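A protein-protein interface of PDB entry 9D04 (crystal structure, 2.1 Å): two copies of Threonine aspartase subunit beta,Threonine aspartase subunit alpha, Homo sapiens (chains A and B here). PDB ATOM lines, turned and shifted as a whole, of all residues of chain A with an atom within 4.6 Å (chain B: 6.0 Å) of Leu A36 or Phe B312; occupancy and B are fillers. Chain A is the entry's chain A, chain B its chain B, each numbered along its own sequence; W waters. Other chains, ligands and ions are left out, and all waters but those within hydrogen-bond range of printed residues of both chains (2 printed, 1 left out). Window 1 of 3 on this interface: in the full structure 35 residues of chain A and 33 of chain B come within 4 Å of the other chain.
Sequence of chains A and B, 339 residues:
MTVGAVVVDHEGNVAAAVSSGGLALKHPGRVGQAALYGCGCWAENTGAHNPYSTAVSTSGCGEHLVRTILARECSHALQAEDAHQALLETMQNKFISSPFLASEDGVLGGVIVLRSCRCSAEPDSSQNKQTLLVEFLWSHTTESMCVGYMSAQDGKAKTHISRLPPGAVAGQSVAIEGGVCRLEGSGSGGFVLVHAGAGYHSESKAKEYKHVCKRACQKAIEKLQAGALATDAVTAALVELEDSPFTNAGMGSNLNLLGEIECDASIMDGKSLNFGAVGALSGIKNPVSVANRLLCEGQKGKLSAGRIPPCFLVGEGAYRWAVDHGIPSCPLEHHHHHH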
ATOM      1  N   GLY A  29      19.957 -15.812 -16.172  1.00  0.00           N
ATOM      2  CA  GLY A  29      19.041 -16.259 -15.149  1.00  0.00           C
ATOM      3  C   GLY A  29      17.581 -16.332 -15.557  1.00  0.00           C
ATOM      4  O   GLY A  29      16.762 -16.782 -14.747  1.00  0.00           O
ATOM      5  N   ARG A  30      17.227 -15.930 -16.778  1.00  0.00           N
ATOM      6  CA  ARG A  30      15.843 -16.059 -17.242  1.00  0.00           C
ATOM      7  C   ARG A  30      15.501 -17.528 -17.445  1.00  0.00           C
ATOM      8  O   ARG A  30      16.153 -18.229 -18.224  1.00  0.00           O
ATOM      9  CB  ARG A  30      15.629 -15.280 -18.542  1.00  0.00           C
ATOM     10  CG  ARG A  30      14.240 -15.467 -19.148  1.00  0.00           C
ATOM     11  CD  ARG A  30      14.054 -14.648 -20.443  1.00  0.00           C
ATOM     12  NE  ARG A  30      12.654 -14.664 -20.873  1.00  0.00           N
ATOM     13  CZ  ARG A  30      12.051 -13.680 -21.537  1.00  0.00           C
ATOM     14  NH1 ARG A  30      12.714 -12.581 -21.874  1.00  0.00           N
ATOM     15  NH2 ARG A  30      10.777 -13.796 -21.873  1.00  0.00           N
ATOM     16  N   VAL A  31      14.460 -17.986 -16.765  1.00  0.00           N
ATOM     17  CA  VAL A  31      14.002 -19.368 -16.835  1.00  0.00           C
ATOM     18  C   VAL A  31      12.651 -19.407 -17.543  1.00  0.00           C
ATOM     19  O   VAL A  31      11.773 -18.584 -17.257  1.00  0.00           O
ATOM     20  CB  VAL A  31      13.915 -19.973 -15.425  1.00  0.00           C
ATOM     21  CG1 VAL A  31      13.246 -21.361 -15.466  1.00  0.00           C
ATOM     22  CG2 VAL A  31      15.340 -20.038 -14.800  1.00  0.00           C
ATOM     23  N   GLY A  32      12.493 -20.344 -18.484  1.00  0.00           N
ATOM     24  CA  GLY A  32      11.292 -20.458 -19.284  1.00  0.00           C
ATOM     25  C   GLY A  32      10.516 -21.741 -19.037  1.00  0.00           C
ATOM     26  O   GLY A  32      10.767 -22.487 -18.085  1.00  0.00           O
ATOM     27  N   GLN A  33       9.600 -22.033 -19.974  1.00  0.00           N
ATOM     28  CA  GLN A  33       8.603 -23.087 -19.774  1.00  0.00           C
ATOM     29  C   GLN A  33       9.214 -24.481 -19.583  1.00  0.00           C
ATOM     30  O   GLN A  33       8.614 -25.322 -18.900  1.00  0.00           O
ATOM     31  CB  GLN A  33       7.621 -23.092 -20.959  1.00  0.00           C
ATOM     32  CG  GLN A  33       7.606 -24.367 -21.814  1.00  0.00           C
ATOM     33  CD  GLN A  33       8.619 -24.327 -22.933  1.00  0.00           C
ATOM     34  OE1 GLN A  33       9.353 -23.367 -23.064  1.00  0.00           O
ATOM     35  NE2 GLN A  33       8.645 -25.362 -23.762  1.00  0.00           N
ATOM     36  N   ALA A  34      10.389 -24.757 -20.171  1.00  0.00           N
ATOM     37  CA  ALA A  34      10.933 -26.116 -20.097  1.00  0.00           C
ATOM     38  C   ALA A  34      11.352 -26.512 -18.681  1.00  0.00           C
ATOM     39  O   ALA A  34      11.558 -27.700 -18.429  1.00  0.00           O
ATOM     40  CB  ALA A  34      12.132 -26.293 -21.047  1.00  0.00           C
ATOM     41  N   ALA A  35      11.478 -25.557 -17.758  1.00  0.00           N
ATOM     42  CA  ALA A  35      11.780 -25.865 -16.366  1.00  0.00           C
ATOM     43  C   ALA A  35      10.564 -25.850 -15.442  1.00  0.00           C
ATOM     44  O   ALA A  35      10.700 -26.247 -14.278  1.00  0.00           O
ATOM     45  CB  ALA A  35      12.817 -24.876 -15.813  1.00  0.00           C
ATOM     46  N   LEU A  36       9.401 -25.393 -15.909  1.00  0.00           N
ATOM     47  CA  LEU A  36       8.307 -24.985 -15.026  1.00  0.00           C
ATOM     48  C   LEU A  36       7.218 -26.046 -14.959  1.00  0.00           C
ATOM     49  O   LEU A  36       6.672 -26.455 -15.994  1.00  0.00           O
ATOM     50  CB  LEU A  36       7.731 -23.637 -15.465  1.00  0.00           C
ATOM     51  CG  LEU A  36       8.691 -22.438 -15.357  1.00  0.00           C
ATOM     52  CD1 LEU A  36       8.031 -21.102 -15.771  1.00  0.00           C
ATOM     53  CD2 LEU A  36       9.198 -22.322 -13.957  1.00  0.00           C
ATOM     54  N   TYR A  37       6.938 -26.508 -13.739  1.00  0.00           N
ATOM     55  CA  TYR A  37       5.876 -27.469 -13.455  1.00  0.00           C
ATOM     56  C   TYR A  37       4.558 -27.073 -14.124  1.00  0.00           C
ATOM     57  O   TYR A  37       4.122 -25.929 -14.024  1.00  0.00           O
ATOM     58  CB  TYR A  37       5.684 -27.559 -11.934  1.00  0.00           C
ATOM     59  CG  TYR A  37       4.765 -28.670 -11.478  1.00  0.00           C
ATOM     60  CD1 TYR A  37       5.146 -29.998 -11.605  1.00  0.00           C
ATOM     61  CD2 TYR A  37       3.545 -28.393 -10.863  1.00  0.00           C
ATOM     62  CE1 TYR A  37       4.327 -31.023 -11.165  1.00  0.00           C
ATOM     63  CE2 TYR A  37       2.717 -29.425 -10.416  1.00  0.00           C
ATOM     64  CZ  TYR A  37       3.120 -30.731 -10.567  1.00  0.00           C
ATOM     65  OH  TYR A  37       2.319 -31.758 -10.126  1.00  0.00           O
ATOM     66  N   GLY A  38       3.923 -28.033 -14.797  1.00  0.00           N
ATOM     67  CA  GLY A  38       2.689 -27.792 -15.512  1.00  0.00           C
ATOM     68  C   GLY A  38       2.851 -27.188 -16.895  1.00  0.00           C
ATOM     69  O   GLY A  38       1.958 -27.344 -17.735  1.00  0.00           O
ATOM     70  N   CYS A  39       3.961 -26.510 -17.174  1.00  0.00           N
ATOM     71  CA  CYS A  39       4.065 -25.734 -18.403  1.00  0.00           C
ATOM     72  C   CYS A  39       4.780 -26.491 -19.516  1.00  0.00           C
ATOM     73  O   CYS A  39       4.252 -26.632 -20.624  1.00  0.00           O
ATOM     74  CB  CYS A  39       4.789 -24.414 -18.102  1.00  0.00           C
ATOM     75  SG  CYS A  39       3.936 -23.418 -16.810  1.00  0.00           S
ATOM     76  N   GLY A  40       5.964 -27.002 -19.226  1.00  0.00           N
ATOM     77  CA  GLY A  40       6.803 -27.624 -20.226  1.00  0.00           C
ATOM     78  C   GLY A  40       6.405 -29.042 -20.575  1.00  0.00           C
ATOM     79  O   GLY A  40       6.490 -29.431 -21.733  1.00  0.00           O
ATOM     80  N   VAL A  66       4.190 -20.672 -20.777  1.00  0.00           N
ATOM     81  CA  VAL A  66       4.090 -20.472 -19.325  1.00  0.00           C
ATOM     82  C   VAL A  66       2.729 -19.903 -18.956  1.00  0.00           C
ATOM     83  O   VAL A  66       2.010 -20.469 -18.125  1.00  0.00           O
ATOM     84  CB  VAL A  66       5.213 -19.555 -18.811  1.00  0.00           C
ATOM     85  CG1 VAL A  66       5.051 -19.319 -17.301  1.00  0.00           C
ATOM     86  CG2 VAL A  66       6.590 -20.142 -19.132  1.00  0.00           C
ATOM     87  N   PHE A 275       8.263 -35.364 -10.276  1.00  0.00           N
ATOM     88  CA  PHE A 275       8.696 -34.331 -11.206  1.00  0.00           C
ATOM     89  C   PHE A 275      10.124 -33.926 -10.859  1.00  0.00           C
ATOM     90  O   PHE A 275      10.472 -33.839  -9.681  1.00  0.00           O
ATOM     91  CB  PHE A 275       7.745 -33.132 -11.088  1.00  0.00           C
ATOM     92  CG  PHE A 275       8.132 -31.928 -11.912  1.00  0.00           C
ATOM     93  CD1 PHE A 275       7.847 -31.872 -13.280  1.00  0.00           C
ATOM     94  CD2 PHE A 275       8.703 -30.812 -11.298  1.00  0.00           C
ATOM     95  CE1 PHE A 275       8.157 -30.746 -14.030  1.00  0.00           C
ATOM     96  CE2 PHE A 275       9.014 -29.678 -12.035  1.00  0.00           C
ATOM     97  CZ  PHE A 275       8.740 -29.642 -13.407  1.00  0.00           C
ATOM     98  N   PHE A 312      13.275 -29.139  -8.039  1.00  0.00           N
ATOM     99  CA  PHE A 312      13.615 -28.047  -8.954  1.00  0.00           C
ATOM    100  C   PHE A 312      14.868 -27.330  -8.450  1.00  0.00           C
ATOM    101  O   PHE A 312      14.804 -26.606  -7.457  1.00  0.00           O
ATOM    102  CB  PHE A 312      12.435 -27.077  -9.060  1.00  0.00           C
ATOM    103  CG  PHE A 312      12.638 -25.936 -10.030  1.00  0.00           C
ATOM    104  CD1 PHE A 312      13.499 -26.048 -11.104  1.00  0.00           C
ATOM    105  CD2 PHE A 312      11.906 -24.756  -9.880  1.00  0.00           C
ATOM    106  CE1 PHE A 312      13.660 -24.997 -11.993  1.00  0.00           C
ATOM    107  CE2 PHE A 312      12.060 -23.706 -10.766  1.00  0.00           C
ATOM    108  CZ  PHE A 312      12.944 -23.825 -11.818  1.00  0.00           C
ATOM    109  N   VAL B  31      14.506 -24.162  -5.611  1.00  0.00           N
ATOM    110  CA  VAL B  31      13.474 -23.147  -5.766  1.00  0.00           C
ATOM    111  C   VAL B  31      12.131 -23.800  -5.458  1.00  0.00           C
ATOM    112  O   VAL B  31      11.828 -24.877  -5.978  1.00  0.00           O
ATOM    113  CB  VAL B  31      13.497 -22.541  -7.179  1.00  0.00           C
ATOM    114  CG1 VAL B  31      12.310 -21.590  -7.362  1.00  0.00           C
ATOM    115  CG2 VAL B  31      14.816 -21.835  -7.431  1.00  0.00           C
ATOM    116  N   ALA B  35       8.063 -19.097  -6.021  1.00  0.00           N
ATOM    117  CA  ALA B  35       8.566 -18.536  -7.260  1.00  0.00           C
ATOM    118  C   ALA B  35       7.822 -19.028  -8.495  1.00  0.00           C
ATOM    119  O   ALA B  35       8.109 -18.537  -9.589  1.00  0.00           O
ATOM    120  CB  ALA B  35      10.071 -18.863  -7.421  1.00  0.00           C
ATOM    121  N   LEU B  36       6.928 -20.013  -8.365  1.00  0.00           N
ATOM    122  CA  LEU B  36       6.443 -20.776  -9.512  1.00  0.00           C
ATOM    123  C   LEU B  36       5.053 -20.294  -9.912  1.00  0.00           C
ATOM    124  O   LEU B  36       4.119 -20.309  -9.097  1.00  0.00           O
ATOM    125  CB  LEU B  36       6.417 -22.277  -9.224  1.00  0.00           C
ATOM    126  CG  LEU B  36       7.761 -22.927  -8.895  1.00  0.00           C
ATOM    127  CD1 LEU B  36       7.620 -24.441  -8.738  1.00  0.00           C
ATOM    128  CD2 LEU B  36       8.803 -22.571  -9.924  1.00  0.00           C
ATOM    129  N   TYR B  37       4.933 -19.868 -11.166  1.00  0.00           N
ATOM    130  CA  TYR B  37       3.659 -19.442 -11.747  1.00  0.00           C
ATOM    131  C   TYR B  37       2.549 -20.441 -11.448  1.00  0.00           C
ATOM    132  O   TYR B  37       2.713 -21.649 -11.644  1.00  0.00           O
ATOM    133  CB  TYR B  37       3.833 -19.306 -13.263  1.00  0.00           C
ATOM    134  CG  TYR B  37       2.673 -18.687 -14.006  1.00  0.00           C
ATOM    135  CD1 TYR B  37       2.377 -17.332 -13.871  1.00  0.00           C
ATOM    136  CD2 TYR B  37       1.900 -19.455 -14.886  1.00  0.00           C
ATOM    137  CE1 TYR B  37       1.311 -16.758 -14.584  1.00  0.00           C
ATOM    138  CE2 TYR B  37       0.841 -18.892 -15.601  1.00  0.00           C
ATOM    139  CZ  TYR B  37       0.551 -17.545 -15.444  1.00  0.00           C
ATOM    140  OH  TYR B  37      -0.494 -16.988 -16.164  1.00  0.00           O
ATOM    141  N   PHE B 275       2.783 -11.150 -14.611  1.00  0.00           N
ATOM    142  CA  PHE B 275       3.389 -11.948 -13.550  1.00  0.00           C
ATOM    143  C   PHE B 275       4.871 -11.609 -13.440  1.00  0.00           C
ATOM    144  O   PHE B 275       5.521 -11.345 -14.456  1.00  0.00           O
ATOM    145  CB  PHE B 275       3.197 -13.440 -13.872  1.00  0.00           C
ATOM    146  CG  PHE B 275       3.851 -14.370 -12.903  1.00  0.00           C
ATOM    147  CD1 PHE B 275       3.234 -14.660 -11.680  1.00  0.00           C
ATOM    148  CD2 PHE B 275       5.065 -14.983 -13.218  1.00  0.00           C
ATOM    149  CE1 PHE B 275       3.823 -15.544 -10.792  1.00  0.00           C
ATOM    150  CE2 PHE B 275       5.662 -15.867 -12.323  1.00  0.00           C
ATOM    151  CZ  PHE B 275       5.046 -16.142 -11.109  1.00  0.00           C
ATOM    152  N   GLY B 276       5.404 -11.611 -12.225  1.00  0.00           N
ATOM    153  CA  GLY B 276       6.841 -11.467 -12.034  1.00  0.00           C
ATOM    154  C   GLY B 276       7.318 -12.392 -10.932  1.00  0.00           C
ATOM    155  O   GLY B 276       6.610 -12.622  -9.953  1.00  0.00           O
ATOM    156  N   ALA B 277       8.543 -12.915 -11.085  1.00  0.00           N
ATOM    157  CA  ALA B 277       9.027 -13.868 -10.092  1.00  0.00           C
ATOM    158  C   ALA B 277      10.554 -13.915 -10.051  1.00  0.00           C
ATOM    159  O   ALA B 277      11.234 -13.691 -11.058  1.00  0.00           O
ATOM    160  CB  ALA B 277       8.459 -15.274 -10.364  1.00  0.00           C
ATOM    161  N   VAL B 278      11.080 -14.225  -8.864  1.00  0.00           N
ATOM    162  CA  VAL B 278      12.493 -14.498  -8.661  1.00  0.00           C
ATOM    163  C   VAL B 278      12.628 -15.799  -7.879  1.00  0.00           C
ATOM    164  O   VAL B 278      11.807 -16.105  -7.008  1.00  0.00           O
ATOM    165  CB  VAL B 278      13.211 -13.342  -7.925  1.00  0.00           C
ATOM    166  CG1 VAL B 278      13.214 -12.072  -8.808  1.00  0.00           C
ATOM    167  CG2 VAL B 278      12.575 -13.086  -6.569  1.00  0.00           C
ATOM    168  N   GLY B 279      13.660 -16.566  -8.195  1.00  0.00           N
ATOM    169  CA  GLY B 279      13.974 -17.763  -7.441  1.00  0.00           C
ATOM    170  C   GLY B 279      15.445 -17.780  -7.085  1.00  0.00           C
ATOM    171  O   GLY B 279      16.291 -17.273  -7.823  1.00  0.00           O
ATOM    172  N   LEU B 294       9.919  -6.738 -12.254  1.00  0.00           N
ATOM    173  CA  LEU B 294       9.788  -7.570 -13.451  1.00  0.00           C
ATOM    174  C   LEU B 294       8.391  -7.446 -14.044  1.00  0.00           C
ATOM    175  O   LEU B 294       8.225  -7.319 -15.266  1.00  0.00           O
ATOM    176  CB  LEU B 294      10.098  -9.029 -13.111  1.00  0.00           C
ATOM    177  CG  LEU B 294      11.574  -9.381 -12.913  1.00  0.00           C
ATOM    178  CD1 LEU B 294      11.725 -10.688 -12.133  1.00  0.00           C
ATOM    179  CD2 LEU B 294      12.303  -9.467 -14.263  1.00  0.00           C
ATOM    180  N   PRO B 310      11.472 -10.555 -19.571  1.00  0.00           N
ATOM    181  CA  PRO B 310      11.448 -11.744 -18.713  1.00  0.00           C
ATOM    182  C   PRO B 310      10.452 -11.570 -17.585  1.00  0.00           C
ATOM    183  O   PRO B 310      10.302 -10.481 -17.027  1.00  0.00           O
ATOM    184  CB  PRO B 310      12.879 -11.822 -18.169  1.00  0.00           C
ATOM    185  CG  PRO B 310      13.343 -10.387 -18.167  1.00  0.00           C
ATOM    186  CD  PRO B 310      12.721  -9.783 -19.416  1.00  0.00           C
ATOM    187  N   CYS B 311       9.792 -12.664 -17.215  1.00  0.00           N
ATOM    188  CA  CYS B 311       8.980 -12.620 -16.019  1.00  0.00           C
ATOM    189  C   CYS B 311       9.574 -13.407 -14.866  1.00  0.00           C
ATOM    190  O   CYS B 311       9.150 -13.196 -13.736  1.00  0.00           O
ATOM    191  CB  CYS B 311       7.554 -13.131 -16.292  1.00  0.00           C
ATOM    192  SG  CYS B 311       7.409 -14.882 -16.670  1.00  0.00           S
ATOM    193  N   PHE B 312      10.564 -14.269 -15.103  1.00  0.00           N
ATOM    194  CA  PHE B 312      11.080 -15.164 -14.061  1.00  0.00           C
ATOM    195  C   PHE B 312      12.602 -15.197 -14.164  1.00  0.00           C
ATOM    196  O   PHE B 312      13.140 -15.729 -15.145  1.00  0.00           O
ATOM    197  CB  PHE B 312      10.481 -16.573 -14.219  1.00  0.00           C
ATOM    198  CG  PHE B 312      10.923 -17.579 -13.150  1.00  0.00           C
ATOM    199  CD1 PHE B 312      11.274 -17.174 -11.865  1.00  0.00           C
ATOM    200  CD2 PHE B 312      10.993 -18.933 -13.456  1.00  0.00           C
ATOM    201  CE1 PHE B 312      11.683 -18.109 -10.888  1.00  0.00           C
ATOM    202  CE2 PHE B 312      11.403 -19.866 -12.517  1.00  0.00           C
ATOM    203  CZ  PHE B 312      11.758 -19.454 -11.218  1.00  0.00           C
ATOM    204  N   LEU B 313      13.304 -14.606 -13.179  1.00  0.00           N
ATOM    205  CA  LEU B 313      14.769 -14.643 -13.113  1.00  0.00           C
ATOM    206  C   LEU B 313      15.234 -15.366 -11.852  1.00  0.00           C
ATOM    207  O   LEU B 313      14.602 -15.267 -10.795  1.00  0.00           O
ATOM    208  CB  LEU B 313      15.398 -13.231 -13.115  1.00  0.00           C
ATOM    209  CG  LEU B 313      15.069 -12.286 -14.276  1.00  0.00           C
ATOM    210  CD1 LEU B 313      15.759 -10.954 -14.074  1.00  0.00           C
ATOM    211  CD2 LEU B 313      15.490 -12.899 -15.600  1.00  0.00           C
ATOM    212  N   VAL B 314      16.374 -16.060 -11.951  1.00  0.00           N
ATOM    213  CA  VAL B 314      16.902 -16.792 -10.810  1.00  0.00           C
ATOM    214  C   VAL B 314      18.372 -16.455 -10.577  1.00  0.00           C
ATOM    215  O   VAL B 314      19.093 -16.003 -11.474  1.00  0.00           O
ATOM    216  CB  VAL B 314      16.730 -18.314 -10.978  1.00  0.00           C
ATOM    217  CG1 VAL B 314      15.237 -18.656 -11.165  1.00  0.00           C
ATOM    218  CG2 VAL B 314      17.613 -18.847 -12.145  1.00  0.00           C
HETATM  219  O   HOH W   1       4.790 -23.591 -12.560  1.00  0.00           O
HETATM  220  O   HOH W   2      12.412 -27.859  -5.350  1.00  0.00           O
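O of Gly A29 is in hydrogen-bond range of N of Val B314.
O of Phe B312 is in hydrogen-bond range of N of Val A31 (3.1 Å).
The backbone carbonyl oxygen of Phe A312 is in hydrogen-bond range of the backbone NH of Val B31 (3.1 Å).
NH1 of Arg A30 sits close to N of Pro B310 (3.3 Å).
The side-chain sulfur of Cys A39 is in hydrogen-bond range of the backbone carbonyl oxygen of Val A66.
O of Ala B277 lies within hydrogen-bond range of N of Leu B313 (3.1 Å).
The backbone NH of Gly B279 is in hydrogen-bond range of the backbone carbonyl oxygen of Leu B313 (3.1 Å).
Among the printed residues, pairs that only touch across the chains: Val A66 with Tyr B37 (3.2 Å), Gly A29 with Leu B313 (3.3 Å), Arg A30 with Phe B312 (3.4 Å), Phe A312 with Leu B36 (3.6 Å), Arg A30 with Leu B313 (3.6 Å), Leu A36 with Phe B312 (3.6 Å), Val A31 with Val B314 (3.7 Å) and Gly A29 with Phe B312 (3.8 Å).
Leu A36 touches one residue of chain B.
Of the printed residues of chain A, Leu B36 touches Phe A312.
Printed residues of chain A within 4 Å of Val B314: Gly A29 (2.9 Å) and Val A31 (3.7 Å).
Printed residues of chain B within 4 Å of Phe A312: Val B31 and Leu B36.
Printed residues of chain B within 4 Å of Gly A29: Phe B312, Leu B313 and Val B314.
The nearest residue of chain B that does not touch Leu A36 is Leu B36 (4.1 Å).
The nearest printed residue of chain B that does not touch Arg A30 is Cys B311 (4.9 Å).
Of the 15 printed residues of chain A, 6 touch a printed residue of chain B.
Printed residues of chain A that touch a printed residue of chain B: Gly A29, Arg A30, Val A31, Leu A36, Val A66 and Phe A312.
Hydrophobic or aromatic side chains of chain A that line the printed part of chain B: Val A31, Leu A36, Val A66 and Phe A312.
Hydrophobic or aromatic side chains of chain B that line the printed part of chain A: Val B31, Leu B36, Tyr B37, Pro B310, Phe B312, Leu B313 and Val B314.
Among the printed residues, no Asp or Glu carboxylate lies within 4 Å of a Lys or Arg side-chain nitrogen of the other chain.
Val A31 touches Phe B312, and with the chains exchanged Phe A312 touches Val B31.
Leu A36 touches Phe B312, and with the chains exchanged Phe A312 touches Leu B36.
Positions printed for both chains: 31, 35, 36, 37, 275 and 312.
Of the 12 pairs that touch across the chains among the printed residues, 4 have their exchanged pair printed and touching as well.
Water W1 bridges O of Tyr A37 (2.8 Å) and O of Tyr B37 (3.0 Å).
Water W2 bridges N of Phe A312 and O of Val B31.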
